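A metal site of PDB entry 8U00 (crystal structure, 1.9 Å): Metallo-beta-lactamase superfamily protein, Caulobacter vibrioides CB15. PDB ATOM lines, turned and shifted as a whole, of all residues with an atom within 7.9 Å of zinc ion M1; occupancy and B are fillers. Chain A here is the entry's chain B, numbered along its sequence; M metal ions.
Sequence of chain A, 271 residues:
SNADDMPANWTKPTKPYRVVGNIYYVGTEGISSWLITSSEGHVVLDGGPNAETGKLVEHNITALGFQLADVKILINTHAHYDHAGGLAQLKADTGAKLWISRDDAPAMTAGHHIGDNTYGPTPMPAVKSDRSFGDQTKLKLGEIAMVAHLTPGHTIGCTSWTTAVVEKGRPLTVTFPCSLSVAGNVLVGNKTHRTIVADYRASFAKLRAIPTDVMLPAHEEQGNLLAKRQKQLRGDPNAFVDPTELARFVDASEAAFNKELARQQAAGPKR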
ATOM      1  N   HIS A  78      26.895  29.550  -4.380  1.00  0.00           N
ATOM      2  CA  HIS A  78      25.700  29.393  -5.204  1.00  0.00           C
ATOM      3  C   HIS A  78      24.503  29.113  -4.314  1.00  0.00           C
ATOM      4  O   HIS A  78      24.643  28.654  -3.168  1.00  0.00           O
ATOM      5  CB  HIS A  78      25.899  28.358  -6.349  1.00  0.00           C
ATOM      6  CG  HIS A  78      25.699  26.917  -5.966  1.00  0.00           C
ATOM      7  ND1 HIS A  78      26.662  26.162  -5.337  1.00  0.00           N
ATOM      8  CD2 HIS A  78      24.662  26.066  -6.224  1.00  0.00           C
ATOM      9  CE1 HIS A  78      26.231  24.930  -5.188  1.00  0.00           C
ATOM     10  NE2 HIS A  78      25.027  24.842  -5.706  1.00  0.00           N
ATOM     11  N   ALA A  79      23.332  29.486  -4.826  1.00  0.00           N
ATOM     12  CA  ALA A  79      22.150  29.710  -4.008  1.00  0.00           C
ATOM     13  C   ALA A  79      21.312  28.451  -3.815  1.00  0.00           C
ATOM     14  O   ALA A  79      20.119  28.561  -3.505  1.00  0.00           O
ATOM     15  CB  ALA A  79      21.289  30.808  -4.620  1.00  0.00           C
ATOM     16  N   HIS A  80      21.892  27.262  -3.974  1.00  0.00           N
ATOM     17  CA  HIS A  80      21.150  26.051  -3.645  1.00  0.00           C
ATOM     18  C   HIS A  80      21.224  25.790  -2.145  1.00  0.00           C
ATOM     19  O   HIS A  80      22.047  26.388  -1.435  1.00  0.00           O
ATOM     20  CB  HIS A  80      21.676  24.875  -4.434  1.00  0.00           C
ATOM     21  CG  HIS A  80      21.269  24.899  -5.877  1.00  0.00           C
ATOM     22  ND1 HIS A  80      21.985  24.264  -6.853  1.00  0.00           N
ATOM     23  CD2 HIS A  80      20.222  25.475  -6.500  1.00  0.00           C
ATOM     24  CE1 HIS A  80      21.390  24.416  -8.019  1.00  0.00           C
ATOM     25  NE2 HIS A  80      20.314  25.163  -7.830  1.00  0.00           N
ATOM     26  N   TYR A  81      20.359  24.893  -1.643  1.00  0.00           N
ATOM     27  CA  TYR A  81      20.167  24.831  -0.194  1.00  0.00           C
ATOM     28  C   TYR A  81      21.440  24.428   0.541  1.00  0.00           C
ATOM     29  O   TYR A  81      21.662  24.900   1.661  1.00  0.00           O
ATOM     30  CB  TYR A  81      19.022  23.869   0.171  1.00  0.00           C
ATOM     31  CG  TYR A  81      19.405  22.412   0.143  1.00  0.00           C
ATOM     32  CD1 TYR A  81      19.946  21.791   1.263  1.00  0.00           C
ATOM     33  CD2 TYR A  81      19.246  21.655  -1.015  1.00  0.00           C
ATOM     34  CE1 TYR A  81      20.309  20.442   1.235  1.00  0.00           C
ATOM     35  CE2 TYR A  81      19.607  20.313  -1.056  1.00  0.00           C
ATOM     36  CZ  TYR A  81      20.129  19.722   0.074  1.00  0.00           C
ATOM     37  OH  TYR A  81      20.493  18.387   0.046  1.00  0.00           O
ATOM     38  N   ASP A  82      22.297  23.582  -0.051  1.00  0.00           N
ATOM     39  CA  ASP A  82      23.402  23.067   0.744  1.00  0.00           C
ATOM     40  C   ASP A  82      24.406  24.159   1.126  1.00  0.00           C
ATOM     41  O   ASP A  82      25.097  24.008   2.126  1.00  0.00           O
ATOM     42  CB  ASP A  82      24.141  21.882   0.083  1.00  0.00           C
ATOM     43  CG  ASP A  82      24.768  22.185  -1.301  1.00  0.00           C
ATOM     44  OD1 ASP A  82      24.302  23.044  -2.086  1.00  0.00           O
ATOM     45  OD2 ASP A  82      25.733  21.454  -1.641  1.00  0.00           O
ATOM     46  N   HIS A  83      24.453  25.258   0.384  1.00  0.00           N
ATOM     47  CA  HIS A  83      25.305  26.394   0.749  1.00  0.00           C
ATOM     48  C   HIS A  83      24.539  27.613   1.208  1.00  0.00           C
ATOM     49  O   HIS A  83      25.092  28.431   1.950  1.00  0.00           O
ATOM     50  CB  HIS A  83      26.179  26.777  -0.437  1.00  0.00           C
ATOM     51  CG  HIS A  83      27.021  25.658  -0.907  1.00  0.00           C
ATOM     52  ND1 HIS A  83      28.059  25.165  -0.154  1.00  0.00           N
ATOM     53  CD2 HIS A  83      26.903  24.848  -1.986  1.00  0.00           C
ATOM     54  CE1 HIS A  83      28.583  24.125  -0.772  1.00  0.00           C
ATOM     55  NE2 HIS A  83      27.922  23.937  -1.897  1.00  0.00           N
ATOM     56  N   HIS A 154      26.831  25.668 -13.231  1.00  0.00           N
ATOM     57  CA  HIS A 154      25.914  24.888 -12.391  1.00  0.00           C
ATOM     58  C   HIS A 154      24.616  25.648 -12.136  1.00  0.00           C
ATOM     59  O   HIS A 154      23.518  25.090 -12.257  1.00  0.00           O
ATOM     60  CB  HIS A 154      26.628  24.533 -11.105  1.00  0.00           C
ATOM     61  CG  HIS A 154      25.810  23.726 -10.175  1.00  0.00           C
ATOM     62  ND1 HIS A 154      25.195  22.546 -10.552  1.00  0.00           N
ATOM     63  CD2 HIS A 154      25.509  23.908  -8.868  1.00  0.00           C
ATOM     64  CE1 HIS A 154      24.551  22.043  -9.526  1.00  0.00           C
ATOM     65  NE2 HIS A 154      24.717  22.832  -8.489  1.00  0.00           N
ATOM     66  N   THR A 155      24.720  26.930 -11.786  1.00  0.00           N
ATOM     67  CA  THR A 155      23.592  27.855 -11.804  1.00  0.00           C
ATOM     68  C   THR A 155      24.034  29.099 -12.553  1.00  0.00           C
ATOM     69  O   THR A 155      25.231  29.339 -12.747  1.00  0.00           O
ATOM     70  CB  THR A 155      23.112  28.269 -10.393  1.00  0.00           C
ATOM     71  OG1 THR A 155      24.082  29.153  -9.805  1.00  0.00           O
ATOM     72  CG2 THR A 155      22.935  27.057  -9.487  1.00  0.00           C
ATOM     73  N   CYS A 158      26.154  31.440  -9.947  1.00  0.00           N
ATOM     74  CA  CYS A 158      27.392  30.988  -9.310  1.00  0.00           C
ATOM     75  C   CYS A 158      28.407  32.119  -9.213  1.00  0.00           C
ATOM     76  O   CYS A 158      28.713  32.767 -10.217  1.00  0.00           O
ATOM     77  CB  CYS A 158      28.009  29.836 -10.094  1.00  0.00           C
ATOM     78  SG  CYS A 158      27.214  28.272  -9.770  1.00  0.00           S
ATOM     79  N   SER A 179      31.337  25.568  -6.349  1.00  0.00           N
ATOM     80  CA  SER A 179      31.583  24.130  -6.275  1.00  0.00           C
ATOM     81  C   SER A 179      31.893  23.503  -7.627  1.00  0.00           C
ATOM     82  O   SER A 179      32.337  22.349  -7.652  1.00  0.00           O
ATOM     83  CB  SER A 179      30.389  23.421  -5.642  1.00  0.00           C
ATOM     84  OG  SER A 179      30.136  23.919  -4.339  1.00  0.00           O
ATOM     85  N   SER A 181      29.975  22.220  -9.682  1.00  0.00           N
ATOM     86  CA  SER A 181      29.177  20.996  -9.717  1.00  0.00           C
ATOM     87  C   SER A 181      28.455  20.807 -11.055  1.00  0.00           C
ATOM     88  O   SER A 181      28.157  21.776 -11.757  1.00  0.00           O
ATOM     89  CB  SER A 181      28.150  21.031  -8.580  1.00  0.00           C
ATOM     90  OG  SER A 181      27.278  19.925  -8.616  1.00  0.00           O
ATOM     91  N   VAL A 182      28.167  19.545 -11.389  1.00  0.00           N
ATOM     92  CA  VAL A 182      27.268  19.210 -12.491  1.00  0.00           C
ATOM     93  C   VAL A 182      26.050  18.427 -12.003  1.00  0.00           C
ATOM     94  O   VAL A 182      25.280  17.924 -12.810  1.00  0.00           O
ATOM     95  CB  VAL A 182      27.991  18.456 -13.614  1.00  0.00           C
ATOM     96  CG1 VAL A 182      29.117  19.304 -14.238  1.00  0.00           C
ATOM     97  CG2 VAL A 182      28.539  17.126 -13.113  1.00  0.00           C
ATOM     98  N   ALA A 183      25.854  18.353 -10.686  1.00  0.00           N
ATOM     99  CA  ALA A 183      24.763  17.562 -10.119  1.00  0.00           C
ATOM    100  C   ALA A 183      23.412  18.048 -10.602  1.00  0.00           C
ATOM    101  O   ALA A 183      23.037  19.215 -10.383  1.00  0.00           O
ATOM    102  CB  ALA A 183      24.826  17.624  -8.594  1.00  0.00           C
ATOM    103  N   GLY A 184      22.664  17.152 -11.256  1.00  0.00           N
ATOM    104  CA  GLY A 184      21.341  17.457 -11.761  1.00  0.00           C
ATOM    105  C   GLY A 184      21.289  18.405 -12.934  1.00  0.00           C
ATOM    106  O   GLY A 184      20.204  18.871 -13.287  1.00  0.00           O
ATOM    107  N   ASN A 185      22.426  18.727 -13.548  1.00  0.00           N
ATOM    108  CA  ASN A 185      22.435  19.641 -14.669  1.00  0.00           C
ATOM    109  C   ASN A 185      22.161  18.900 -15.967  1.00  0.00           C
ATOM    110  O   ASN A 185      22.668  17.795 -16.201  1.00  0.00           O
ATOM    111  CB  ASN A 185      23.780  20.379 -14.746  1.00  0.00           C
ATOM    112  CG  ASN A 185      23.923  21.423 -13.660  1.00  0.00           C
ATOM    113  OD1 ASN A 185      24.710  21.260 -12.737  1.00  0.00           O
ATOM    114  ND2 ASN A 185      23.156  22.495 -13.767  1.00  0.00           N
ATOM    115  N   HIS A 219      33.081  22.719  -0.364  1.00  0.00           N
ATOM    116  CA  HIS A 219      32.969  21.374   0.212  1.00  0.00           C
ATOM    117  C   HIS A 219      34.309  20.916   0.774  1.00  0.00           C
ATOM    118  O   HIS A 219      35.347  21.100   0.133  1.00  0.00           O
ATOM    119  CB  HIS A 219      32.493  20.362  -0.837  1.00  0.00           C
ATOM    120  CG  HIS A 219      31.022  20.368  -1.043  1.00  0.00           C
ATOM    121  ND1 HIS A 219      30.163  19.660  -0.241  1.00  0.00           N
ATOM    122  CD2 HIS A 219      30.246  21.001  -1.960  1.00  0.00           C
ATOM    123  CE1 HIS A 219      28.915  19.841  -0.644  1.00  0.00           C
ATOM    124  NE2 HIS A 219      28.945  20.638  -1.699  1.00  0.00           N
HETATM  125 ZN    ZN M   1      23.820  23.091  -6.474  1.00  0.00          ZN
HETATM  126 ZN    ZN M   2      27.435  21.919  -2.649  1.00  0.00          ZN
HETATM  127 ZN    ZN M   3      29.110  27.074  -9.374  1.00  0.00          ZN
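Zinc ion M1 is bound by a ring nitrogen (ND1) of His 80, a ring nitrogen (NE2) of His 154 and a ring nitrogen (NE2) of His 78. Zinc ion M1 has three donor atoms within binding distance.
Within 4 Å of zinc ion M1: His 78, His 80 and His 154.
A ring nitrogen (ND1) of His 154 sits close to the backbone carbonyl oxygen of Ser 181 (3.3 Å). OD1 of Asn 185 sits at hydrogen-bond distance from ND1 of His 154.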
